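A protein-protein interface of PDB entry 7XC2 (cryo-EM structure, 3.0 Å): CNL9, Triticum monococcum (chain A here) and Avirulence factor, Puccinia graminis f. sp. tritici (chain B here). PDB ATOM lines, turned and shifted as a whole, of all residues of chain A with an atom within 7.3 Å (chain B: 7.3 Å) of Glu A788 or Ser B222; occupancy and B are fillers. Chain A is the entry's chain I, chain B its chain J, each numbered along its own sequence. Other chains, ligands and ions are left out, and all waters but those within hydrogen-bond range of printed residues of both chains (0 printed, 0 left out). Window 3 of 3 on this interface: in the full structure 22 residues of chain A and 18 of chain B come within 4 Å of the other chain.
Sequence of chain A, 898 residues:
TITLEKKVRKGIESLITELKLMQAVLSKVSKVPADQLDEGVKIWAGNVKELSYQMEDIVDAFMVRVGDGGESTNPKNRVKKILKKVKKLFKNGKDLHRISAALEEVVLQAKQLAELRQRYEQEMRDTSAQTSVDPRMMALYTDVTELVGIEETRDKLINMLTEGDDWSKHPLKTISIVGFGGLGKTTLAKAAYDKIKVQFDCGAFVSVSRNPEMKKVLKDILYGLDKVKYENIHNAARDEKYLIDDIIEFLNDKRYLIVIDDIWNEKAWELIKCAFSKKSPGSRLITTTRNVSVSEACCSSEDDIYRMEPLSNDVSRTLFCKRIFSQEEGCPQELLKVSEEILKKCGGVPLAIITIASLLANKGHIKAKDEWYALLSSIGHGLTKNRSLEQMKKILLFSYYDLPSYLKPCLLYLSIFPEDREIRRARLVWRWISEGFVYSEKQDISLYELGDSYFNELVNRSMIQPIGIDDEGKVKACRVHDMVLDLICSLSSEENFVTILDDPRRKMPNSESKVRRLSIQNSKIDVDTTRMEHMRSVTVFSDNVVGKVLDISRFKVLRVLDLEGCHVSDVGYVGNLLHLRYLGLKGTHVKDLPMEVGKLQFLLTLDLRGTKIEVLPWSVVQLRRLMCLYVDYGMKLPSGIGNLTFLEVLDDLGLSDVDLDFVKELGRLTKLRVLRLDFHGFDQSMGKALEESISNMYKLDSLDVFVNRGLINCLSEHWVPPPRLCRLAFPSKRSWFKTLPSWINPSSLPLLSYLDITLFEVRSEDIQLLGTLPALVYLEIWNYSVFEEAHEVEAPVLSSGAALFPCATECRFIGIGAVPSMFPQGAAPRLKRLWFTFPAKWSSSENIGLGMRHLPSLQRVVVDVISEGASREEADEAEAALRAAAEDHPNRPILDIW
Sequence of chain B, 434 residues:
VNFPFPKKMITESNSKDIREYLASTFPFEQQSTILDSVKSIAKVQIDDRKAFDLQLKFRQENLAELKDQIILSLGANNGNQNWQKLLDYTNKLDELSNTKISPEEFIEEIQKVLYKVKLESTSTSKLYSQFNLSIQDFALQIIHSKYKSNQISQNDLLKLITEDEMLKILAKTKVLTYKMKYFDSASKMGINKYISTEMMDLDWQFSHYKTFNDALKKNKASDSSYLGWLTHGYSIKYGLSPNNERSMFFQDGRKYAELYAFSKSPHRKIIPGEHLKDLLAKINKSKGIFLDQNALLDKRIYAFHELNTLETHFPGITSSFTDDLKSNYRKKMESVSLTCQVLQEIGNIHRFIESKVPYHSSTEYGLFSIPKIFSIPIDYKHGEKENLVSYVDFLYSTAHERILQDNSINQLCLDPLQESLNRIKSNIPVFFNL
The guanidinium group (NH2) of Arg A709 is in salt-bridge range of the side-chain carboxylate (OD1) of Asp B223 (2.5 Å).
The guanidinium group (NH2) of Arg A734 is in salt-bridge range of the side-chain carboxylate (OD1) of Asp B223, 3.1 Å away.
The guanidinium group (NH1) of Arg A734 lies within hydrogen-bond range of the side-chain hydroxyl (OH) of Tyr B256 (2.6 Å).
OE1 of Glu A788 is in hydrogen-bond range of OG of Ser B222 (3.1 Å).
The side-chain hydroxyl (OH) of Tyr B260 is in hydrogen-bond range of the side-chain carboxylate (OE1) of Glu A788 (3.4 Å).
NH2 of Arg A734 is in salt-bridge range of OE2 of Glu A788, 3.2 Å away.
Among the printed residues, merely in contact across the chains: Arg A709 with Tyr B226 (3.6 Å), Lys A733 with Tyr B260 (3.7 Å), Arg A734 with Tyr B260 (3.7 Å) and Phe A787 with Lys B264 (3.9 Å).
Printed residues of chain B within 4 Å of Arg A709: Asp B223 (2.5 Å) and Tyr B226 (3.6 Å).
Of chain B, only Ser B222 and Tyr B260 come within 4 Å of Glu A788.
Lys B220 touches none of the printed residues of chain A.
No residue of chain A comes within 4 Å of Ala B221.
Printed residues of chain A within 4 Å of Tyr B260: Lys A733 (3.7 Å), Arg A734 (3.7 Å) and Glu A788 (3.4 Å).
The nearest residue of chain B that does not touch Glu A788 is Lys B264 (4.8 Å).
The nearest residue of chain A that does not touch Ser B222 is Arg A734 (4.1 Å).
Of the 16 printed residues of chain B, 6 touch a printed residue of chain A.
Printed residues of chain B that touch a printed residue of chain A: Ser B222, Asp B223, Tyr B226, Tyr B256, Tyr B260 and Lys B264.
Hydrophobic or aromatic side chains of chain A within 4 Å of the printed part of chain B: Phe A787.
Among the printed residues, Asp or Glu carboxylates within 4 Å of a Lys or Arg side-chain nitrogen of the other chain: Arg A709 with Asp B223 (2.5 Å) and Arg A734 with Asp B223 (3.1 Å).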
ATOM      1  N   ARG A 709       5.538  -2.643   4.574  1.00  0.00           N
ATOM      2  CA  ARG A 709       5.135  -1.281   4.884  1.00  0.00           C
ATOM      3  C   ARG A 709       6.081  -0.697   5.920  1.00  0.00           C
ATOM      4  O   ARG A 709       7.018  -1.352   6.381  1.00  0.00           O
ATOM      5  CB  ARG A 709       3.696  -1.236   5.405  1.00  0.00           C
ATOM      6  CG  ARG A 709       2.656  -1.737   4.435  1.00  0.00           C
ATOM      7  CD  ARG A 709       1.362  -2.056   5.147  1.00  0.00           C
ATOM      8  NE  ARG A 709       0.217  -1.882   4.262  1.00  0.00           N
ATOM      9  CZ  ARG A 709      -0.547  -0.796   4.241  1.00  0.00           C
ATOM     10  NH1 ARG A 709      -0.292   0.209   5.064  1.00  0.00           N
ATOM     11  NH2 ARG A 709      -1.567  -0.717   3.400  1.00  0.00           N
ATOM     12  N   LYS A 733       8.488  -0.123  -2.548  1.00  0.00           N
ATOM     13  CA  LYS A 733       7.749   1.033  -3.060  1.00  0.00           C
ATOM     14  C   LYS A 733       6.702   1.556  -2.092  1.00  0.00           C
ATOM     15  O   LYS A 733       6.059   2.564  -2.392  1.00  0.00           O
ATOM     16  CB  LYS A 733       7.057   0.761  -4.401  1.00  0.00           C
ATOM     17  CG  LYS A 733       7.989   0.308  -5.488  1.00  0.00           C
ATOM     18  CD  LYS A 733       8.953   1.406  -5.851  1.00  0.00           C
ATOM     19  CE  LYS A 733       9.874   0.959  -6.962  1.00  0.00           C
ATOM     20  NZ  LYS A 733      11.268   0.798  -6.483  1.00  0.00           N
ATOM     21  N   ARG A 734       6.502   0.910  -0.949  1.00  0.00           N
ATOM     22  CA  ARG A 734       5.624   1.429   0.085  1.00  0.00           C
ATOM     23  C   ARG A 734       6.271   1.466   1.453  1.00  0.00           C
ATOM     24  O   ARG A 734       5.619   1.901   2.406  1.00  0.00           O
ATOM     25  CB  ARG A 734       4.335   0.604   0.176  1.00  0.00           C
ATOM     26  CG  ARG A 734       3.388   0.833  -0.973  1.00  0.00           C
ATOM     27  CD  ARG A 734       2.005   0.321  -0.654  1.00  0.00           C
ATOM     28  NE  ARG A 734       1.405   1.050   0.452  1.00  0.00           N
ATOM     29  CZ  ARG A 734       0.138   0.920   0.821  1.00  0.00           C
ATOM     30  NH1 ARG A 734      -0.658   0.090   0.165  1.00  0.00           N
ATOM     31  NH2 ARG A 734      -0.333   1.618   1.842  1.00  0.00           N
ATOM     32  N   TRP A 736       9.497   3.211   3.204  1.00  0.00           N
ATOM     33  CA  TRP A 736      10.457   4.257   2.902  1.00  0.00           C
ATOM     34  C   TRP A 736      11.691   4.161   3.781  1.00  0.00           C
ATOM     35  O   TRP A 736      11.656   3.600   4.877  1.00  0.00           O
ATOM     36  CB  TRP A 736       9.819   5.626   3.115  1.00  0.00           C
ATOM     37  CG  TRP A 736       9.398   5.808   4.534  1.00  0.00           C
ATOM     38  CD1 TRP A 736      10.120   6.378   5.537  1.00  0.00           C
ATOM     39  CD2 TRP A 736       8.166   5.386   5.119  1.00  0.00           C
ATOM     40  NE1 TRP A 736       9.412   6.350   6.707  1.00  0.00           N
ATOM     41  CE2 TRP A 736       8.207   5.744   6.477  1.00  0.00           C
ATOM     42  CE3 TRP A 736       7.030   4.747   4.625  1.00  0.00           C
ATOM     43  CZ2 TRP A 736       7.156   5.483   7.345  1.00  0.00           C
ATOM     44  CZ3 TRP A 736       5.991   4.490   5.487  1.00  0.00           C
ATOM     45  CH2 TRP A 736       6.060   4.855   6.832  1.00  0.00           C
ATOM     46  N   ASN A 783       9.575   9.243  -4.323  1.00  0.00           N
ATOM     47  CA  ASN A 783       9.303  10.169  -3.230  1.00  0.00           C
ATOM     48  C   ASN A 783       8.016   9.718  -2.552  1.00  0.00           C
ATOM     49  O   ASN A 783       6.924   9.889  -3.101  1.00  0.00           O
ATOM     50  CB  ASN A 783       9.189  11.602  -3.740  1.00  0.00           C
ATOM     51  CG  ASN A 783       9.265  12.618  -2.629  1.00  0.00           C
ATOM     52  OD1 ASN A 783       9.354  12.266  -1.456  1.00  0.00           O
ATOM     53  ND2 ASN A 783       9.239  13.891  -2.992  1.00  0.00           N
ATOM     54  N   TYR A 784       8.151   9.144  -1.357  1.00  0.00           N
ATOM     55  CA  TYR A 784       7.012   8.522  -0.694  1.00  0.00           C
ATOM     56  C   TYR A 784       5.987   9.549  -0.243  1.00  0.00           C
ATOM     57  O   TYR A 784       4.789   9.248  -0.196  1.00  0.00           O
ATOM     58  CB  TYR A 784       7.504   7.702   0.495  1.00  0.00           C
ATOM     59  CG  TYR A 784       6.410   7.172   1.378  1.00  0.00           C
ATOM     60  CD1 TYR A 784       5.722   6.023   1.042  1.00  0.00           C
ATOM     61  CD2 TYR A 784       6.072   7.814   2.557  1.00  0.00           C
ATOM     62  CE1 TYR A 784       4.731   5.530   1.846  1.00  0.00           C
ATOM     63  CE2 TYR A 784       5.077   7.328   3.366  1.00  0.00           C
ATOM     64  CZ  TYR A 784       4.409   6.186   3.005  1.00  0.00           C
ATOM     65  OH  TYR A 784       3.412   5.688   3.805  1.00  0.00           O
ATOM     66  N   SER A 785       6.435  10.753   0.101  1.00  0.00           N
ATOM     67  CA  SER A 785       5.535  11.757   0.650  1.00  0.00           C
ATOM     68  C   SER A 785       4.592  12.323  -0.402  1.00  0.00           C
ATOM     69  O   SER A 785       3.478  12.734  -0.073  1.00  0.00           O
ATOM     70  CB  SER A 785       6.345  12.878   1.288  1.00  0.00           C
ATOM     71  OG  SER A 785       7.245  13.443   0.351  1.00  0.00           O
ATOM     72  N   VAL A 786       5.014  12.354  -1.665  1.00  0.00           N
ATOM     73  CA  VAL A 786       4.173  12.944  -2.699  1.00  0.00           C
ATOM     74  C   VAL A 786       2.891  12.147  -2.873  1.00  0.00           C
ATOM     75  O   VAL A 786       1.796  12.715  -2.944  1.00  0.00           O
ATOM     76  CB  VAL A 786       4.951  13.047  -4.018  1.00  0.00           C
ATOM     77  CG1 VAL A 786       4.002  13.342  -5.158  1.00  0.00           C
ATOM     78  CG2 VAL A 786       6.012  14.117  -3.913  1.00  0.00           C
ATOM     79  N   PHE A 787       3.000  10.822  -2.927  1.00  0.00           N
ATOM     80  CA  PHE A 787       1.851   9.972  -3.213  1.00  0.00           C
ATOM     81  C   PHE A 787       1.056   9.643  -1.954  1.00  0.00           C
ATOM     82  O   PHE A 787      -0.136   9.948  -1.867  1.00  0.00           O
ATOM     83  CB  PHE A 787       2.319   8.687  -3.900  1.00  0.00           C
ATOM     84  CG  PHE A 787       3.041   8.924  -5.187  1.00  0.00           C
ATOM     85  CD1 PHE A 787       2.345   9.014  -6.374  1.00  0.00           C
ATOM     86  CD2 PHE A 787       4.415   9.054  -5.214  1.00  0.00           C
ATOM     87  CE1 PHE A 787       3.002   9.232  -7.564  1.00  0.00           C
ATOM     88  CE2 PHE A 787       5.077   9.270  -6.403  1.00  0.00           C
ATOM     89  CZ  PHE A 787       4.370   9.359  -7.577  1.00  0.00           C
ATOM     90  N   GLU A 788       1.705   9.022  -0.969  1.00  0.00           N
ATOM     91  CA  GLU A 788       0.970   8.546   0.196  1.00  0.00           C
ATOM     92  C   GLU A 788       0.544   9.697   1.093  1.00  0.00           C
ATOM     93  O   GLU A 788      -0.596   9.729   1.568  1.00  0.00           O
ATOM     94  CB  GLU A 788       1.808   7.531   0.967  1.00  0.00           C
ATOM     95  CG  GLU A 788       1.762   6.138   0.363  1.00  0.00           C
ATOM     96  CD  GLU A 788       0.365   5.548   0.349  1.00  0.00           C
ATOM     97  OE1 GLU A 788      -0.405   5.840  -0.591  1.00  0.00           O
ATOM     98  OE2 GLU A 788       0.035   4.789   1.282  1.00  0.00           O
ATOM     99  N   GLU A 789       1.438  10.645   1.346  1.00  0.00           N
ATOM    100  CA  GLU A 789       1.055  11.872   2.029  1.00  0.00           C
ATOM    101  C   GLU A 789       0.482  12.841   0.998  1.00  0.00           C
ATOM    102  O   GLU A 789       0.197  12.472  -0.145  1.00  0.00           O
ATOM    103  CB  GLU A 789       2.242  12.453   2.787  1.00  0.00           C
ATOM    104  CG  GLU A 789       2.898  11.474   3.736  1.00  0.00           C
ATOM    105  CD  GLU A 789       2.006  11.112   4.904  1.00  0.00           C
ATOM    106  OE1 GLU A 789       1.068  11.882   5.199  1.00  0.00           O
ATOM    107  OE2 GLU A 789       2.241  10.056   5.529  1.00  0.00           O
ATOM    108  N   ALA A 790       0.304  14.101   1.385  1.00  0.00           N
ATOM    109  CA  ALA A 790      -0.284  15.098   0.499  1.00  0.00           C
ATOM    110  C   ALA A 790       0.695  16.207   0.135  1.00  0.00           C
ATOM    111  O   ALA A 790       0.270  17.287  -0.281  1.00  0.00           O
ATOM    112  CB  ALA A 790      -1.541  15.689   1.132  1.00  0.00           C
ATOM    113  N   HIS A 791       1.993  15.963   0.278  1.00  0.00           N
ATOM    114  CA  HIS A 791       2.970  16.974  -0.083  1.00  0.00           C
ATOM    115  C   HIS A 791       2.924  17.239  -1.587  1.00  0.00           C
ATOM    116  O   HIS A 791       2.301  16.508  -2.359  1.00  0.00           O
ATOM    117  CB  HIS A 791       4.369  16.542   0.345  1.00  0.00           C
ATOM    118  CG  HIS A 791       4.505  16.321   1.818  1.00  0.00           C
ATOM    119  ND1 HIS A 791       5.462  16.954   2.579  1.00  0.00           N
ATOM    120  CD2 HIS A 791       3.803  15.540   2.671  1.00  0.00           C
ATOM    121  CE1 HIS A 791       5.346  16.570   3.838  1.00  0.00           C
ATOM    122  NE2 HIS A 791       4.346  15.712   3.920  1.00  0.00           N
ATOM    123  N   LEU B 216     -12.422   3.906   3.845  1.00  0.00           N
ATOM    124  CA  LEU B 216     -11.126   3.937   3.184  1.00  0.00           C
ATOM    125  C   LEU B 216     -11.220   4.644   1.839  1.00  0.00           C
ATOM    126  O   LEU B 216     -10.325   5.416   1.474  1.00  0.00           O
ATOM    127  CB  LEU B 216     -10.577   2.519   3.055  1.00  0.00           C
ATOM    128  CG  LEU B 216     -10.386   1.967   4.472  1.00  0.00           C
ATOM    129  CD1 LEU B 216     -10.006   0.496   4.487  1.00  0.00           C
ATOM    130  CD2 LEU B 216      -9.361   2.798   5.224  1.00  0.00           C
ATOM    131  N   ASN B 219     -10.565   8.156   2.444  1.00  0.00           N
ATOM    132  CA  ASN B 219      -9.326   8.751   2.924  1.00  0.00           C
ATOM    133  C   ASN B 219      -8.090   8.232   2.200  1.00  0.00           C
ATOM    134  O   ASN B 219      -7.252   9.021   1.760  1.00  0.00           O
ATOM    135  CB  ASN B 219      -9.207   8.496   4.424  1.00  0.00           C
ATOM    136  CG  ASN B 219     -10.350   9.111   5.196  1.00  0.00           C
ATOM    137  OD1 ASN B 219     -10.630  10.299   5.065  1.00  0.00           O
ATOM    138  ND2 ASN B 219     -11.044   8.294   5.982  1.00  0.00           N
ATOM    139  N   LYS B 220      -7.950   6.915   2.093  1.00  0.00           N
ATOM    140  CA  LYS B 220      -6.756   6.308   1.513  1.00  0.00           C
ATOM    141  C   LYS B 220      -7.222   5.207   0.568  1.00  0.00           C
ATOM    142  O   LYS B 220      -7.554   4.104   1.011  1.00  0.00           O
ATOM    143  CB  LYS B 220      -5.844   5.759   2.602  1.00  0.00           C
ATOM    144  CG  LYS B 220      -5.367   6.810   3.587  1.00  0.00           C
ATOM    145  CD  LYS B 220      -4.350   6.241   4.557  1.00  0.00           C
ATOM    146  CE  LYS B 220      -3.766   7.336   5.432  1.00  0.00           C
ATOM    147  NZ  LYS B 220      -2.617   6.843   6.241  1.00  0.00           N
ATOM    148  N   ALA B 221      -7.251   5.508  -0.728  1.00  0.00           N
ATOM    149  CA  ALA B 221      -7.682   4.505  -1.693  1.00  0.00           C
ATOM    150  C   ALA B 221      -6.701   3.346  -1.767  1.00  0.00           C
ATOM    151  O   ALA B 221      -7.109   2.204  -2.025  1.00  0.00           O
ATOM    152  CB  ALA B 221      -7.853   5.138  -3.071  1.00  0.00           C
ATOM    153  N   SER B 222      -5.412   3.623  -1.554  1.00  0.00           N
ATOM    154  CA  SER B 222      -4.407   2.569  -1.609  1.00  0.00           C
ATOM    155  C   SER B 222      -4.759   1.431  -0.669  1.00  0.00           C
ATOM    156  O   SER B 222      -4.732   0.258  -1.061  1.00  0.00           O
ATOM    157  CB  SER B 222      -3.034   3.139  -1.267  1.00  0.00           C
ATOM    158  OG  SER B 222      -2.909   4.467  -1.735  1.00  0.00           O
ATOM    159  N   ASP B 223      -5.110   1.759   0.572  1.00  0.00           N
ATOM    160  CA  ASP B 223      -5.454   0.722   1.533  1.00  0.00           C
ATOM    161  C   ASP B 223      -6.738   0.006   1.156  1.00  0.00           C
ATOM    162  O   ASP B 223      -6.881  -1.183   1.442  1.00  0.00           O
ATOM    163  CB  ASP B 223      -5.571   1.322   2.927  1.00  0.00           C
ATOM    164  CG  ASP B 223      -4.226   1.534   3.573  1.00  0.00           C
ATOM    165  OD1 ASP B 223      -3.214   1.132   2.965  1.00  0.00           O
ATOM    166  OD2 ASP B 223      -4.175   2.103   4.681  1.00  0.00           O
ATOM    167  N   SER B 224      -7.672   0.693   0.502  1.00  0.00           N
ATOM    168  CA  SER B 224      -8.890   0.025   0.061  1.00  0.00           C
ATOM    169  C   SER B 224      -8.572  -1.037  -0.979  1.00  0.00           C
ATOM    170  O   SER B 224      -9.036  -2.183  -0.889  1.00  0.00           O
ATOM    171  CB  SER B 224      -9.869   1.046  -0.508  1.00  0.00           C
ATOM    172  OG  SER B 224      -9.484   1.417  -1.818  1.00  0.00           O
ATOM    173  N   SER B 225      -7.776  -0.667  -1.983  1.00  0.00           N
ATOM    174  CA  SER B 225      -7.386  -1.634  -3.000  1.00  0.00           C
ATOM    175  C   SER B 225      -6.591  -2.776  -2.386  1.00  0.00           C
ATOM    176  O   SER B 225      -6.754  -3.940  -2.771  1.00  0.00           O
ATOM    177  CB  SER B 225      -6.571  -0.942  -4.087  1.00  0.00           C
ATOM    178  OG  SER B 225      -7.368   0.002  -4.775  1.00  0.00           O
ATOM    179  N   TYR B 226      -5.725  -2.459  -1.425  1.00  0.00           N
ATOM    180  CA  TYR B 226      -4.970  -3.492  -0.730  1.00  0.00           C
ATOM    181  C   TYR B 226      -5.895  -4.443   0.011  1.00  0.00           C
ATOM    182  O   TYR B 226      -5.687  -5.661   0.001  1.00  0.00           O
ATOM    183  CB  TYR B 226      -3.991  -2.838   0.236  1.00  0.00           C
ATOM    184  CG  TYR B 226      -3.145  -3.806   1.007  1.00  0.00           C
ATOM    185  CD1 TYR B 226      -2.317  -4.699   0.356  1.00  0.00           C
ATOM    186  CD2 TYR B 226      -3.164  -3.820   2.390  1.00  0.00           C
ATOM    187  CE1 TYR B 226      -1.537  -5.579   1.059  1.00  0.00           C
ATOM    188  CE2 TYR B 226      -2.387  -4.696   3.101  1.00  0.00           C
ATOM    189  CZ  TYR B 226      -1.575  -5.575   2.431  1.00  0.00           C
ATOM    190  OH  TYR B 226      -0.793  -6.458   3.133  1.00  0.00           O
ATOM    191  N   LEU B 227      -6.930  -3.905   0.649  1.00  0.00           N
ATOM    192  CA  LEU B 227      -7.881  -4.744   1.362  1.00  0.00           C
ATOM    193  C   LEU B 227      -8.625  -5.658   0.403  1.00  0.00           C
ATOM    194  O   LEU B 227      -8.871  -6.828   0.713  1.00  0.00           O
ATOM    195  CB  LEU B 227      -8.856  -3.871   2.143  1.00  0.00           C
ATOM    196  CG  LEU B 227      -9.900  -4.623   2.960  1.00  0.00           C
ATOM    197  CD1 LEU B 227      -9.225  -5.603   3.896  1.00  0.00           C
ATOM    198  CD2 LEU B 227     -10.765  -3.652   3.734  1.00  0.00           C
ATOM    199  N   GLY B 228      -8.984  -5.145  -0.771  1.00  0.00           N
ATOM    200  CA  GLY B 228      -9.643  -5.994  -1.752  1.00  0.00           C
ATOM    201  C   GLY B 228      -8.741  -7.111  -2.247  1.00  0.00           C
ATOM    202  O   GLY B 228      -9.148  -8.278  -2.328  1.00  0.00           O
ATOM    203  N   TYR B 256       1.601  -7.620  -5.131  1.00  0.00           N
ATOM    204  CA  TYR B 256       0.948  -6.375  -4.766  1.00  0.00           C
ATOM    205  C   TYR B 256       1.880  -5.190  -4.947  1.00  0.00           C
ATOM    206  O   TYR B 256       1.428  -4.097  -5.299  1.00  0.00           O
ATOM    207  CB  TYR B 256       0.455  -6.431  -3.328  1.00  0.00           C
ATOM    208  CG  TYR B 256      -0.111  -5.117  -2.881  1.00  0.00           C
ATOM    209  CD1 TYR B 256      -1.340  -4.687  -3.341  1.00  0.00           C
ATOM    210  CD2 TYR B 256       0.590  -4.293  -2.025  1.00  0.00           C
ATOM    211  CE1 TYR B 256      -1.860  -3.485  -2.949  1.00  0.00           C
ATOM    212  CE2 TYR B 256       0.077  -3.089  -1.627  1.00  0.00           C
ATOM    213  CZ  TYR B 256      -1.148  -2.688  -2.093  1.00  0.00           C
ATOM    214  OH  TYR B 256      -1.669  -1.482  -1.698  1.00  0.00           O
ATOM    215  N   TYR B 260       0.854  -2.004  -7.204  1.00  0.00           N
ATOM    216  CA  TYR B 260       0.866  -0.645  -6.675  1.00  0.00           C
ATOM    217  C   TYR B 260       1.766   0.257  -7.504  1.00  0.00           C
ATOM    218  O   TYR B 260       1.388   1.389  -7.838  1.00  0.00           O
ATOM    219  CB  TYR B 260       1.324  -0.669  -5.221  1.00  0.00           C
ATOM    220  CG  TYR B 260       1.455   0.687  -4.582  1.00  0.00           C
ATOM    221  CD1 TYR B 260       2.622   1.422  -4.697  1.00  0.00           C
ATOM    222  CD2 TYR B 260       0.417   1.223  -3.844  1.00  0.00           C
ATOM    223  CE1 TYR B 260       2.744   2.656  -4.110  1.00  0.00           C
ATOM    224  CE2 TYR B 260       0.532   2.456  -3.253  1.00  0.00           C
ATOM    225  CZ  TYR B 260       1.696   3.168  -3.389  1.00  0.00           C
ATOM    226  OH  TYR B 260       1.814   4.400  -2.800  1.00  0.00           O
ATOM    227  N   SER B 263       0.039   1.222 -10.441  1.00  0.00           N
ATOM    228  CA  SER B 263      -1.087   2.092 -10.134  1.00  0.00           C
ATOM    229  C   SER B 263      -0.652   3.528  -9.902  1.00  0.00           C
ATOM    230  O   SER B 263      -1.445   4.450 -10.106  1.00  0.00           O
ATOM    231  CB  SER B 263      -1.830   1.573  -8.909  1.00  0.00           C
ATOM    232  OG  SER B 263      -2.842   2.480  -8.521  1.00  0.00           O
ATOM    233  N   LYS B 264       0.587   3.740  -9.468  1.00  0.00           N
ATOM    234  CA  LYS B 264       1.038   5.107  -9.242  1.00  0.00           C
ATOM    235  C   LYS B 264       1.649   5.751 -10.478  1.00  0.00           C
ATOM    236  O   LYS B 264       1.456   6.950 -10.694  1.00  0.00           O
ATOM    237  CB  LYS B 264       2.036   5.154  -8.088  1.00  0.00           C
ATOM    238  CG  LYS B 264       1.367   5.065  -6.737  1.00  0.00           C
ATOM    239  CD  LYS B 264       0.079   5.861  -6.733  1.00  0.00           C
ATOM    240  CE  LYS B 264      -0.634   5.752  -5.405  1.00  0.00           C
ATOM    241  NZ  LYS B 264      -1.855   6.599  -5.384  1.00  0.00           N
ATOM    242  N   PHE B 314      -7.649  -2.389  -9.527  1.00  0.00           N
ATOM    243  CA  PHE B 314      -6.573  -1.713 -10.247  1.00  0.00           C
ATOM    244  C   PHE B 314      -7.065  -1.384 -11.643  1.00  0.00           C
ATOM    245  O   PHE B 314      -6.871  -2.179 -12.579  1.00  0.00           O
ATOM    246  CB  PHE B 314      -5.322  -2.581 -10.298  1.00  0.00           C
ATOM    247  CG  PHE B 314      -4.862  -3.035  -8.952  1.00  0.00           C
ATOM    248  CD1 PHE B 314      -4.083  -2.215  -8.164  1.00  0.00           C
ATOM    249  CD2 PHE B 314      -5.227  -4.271  -8.463  1.00  0.00           C
ATOM    250  CE1 PHE B 314      -3.664  -2.625  -6.922  1.00  0.00           C
ATOM    251  CE2 PHE B 314      -4.812  -4.685  -7.221  1.00  0.00           C
ATOM    252  CZ  PHE B 314      -4.030  -3.860  -6.450  1.00  0.00           C
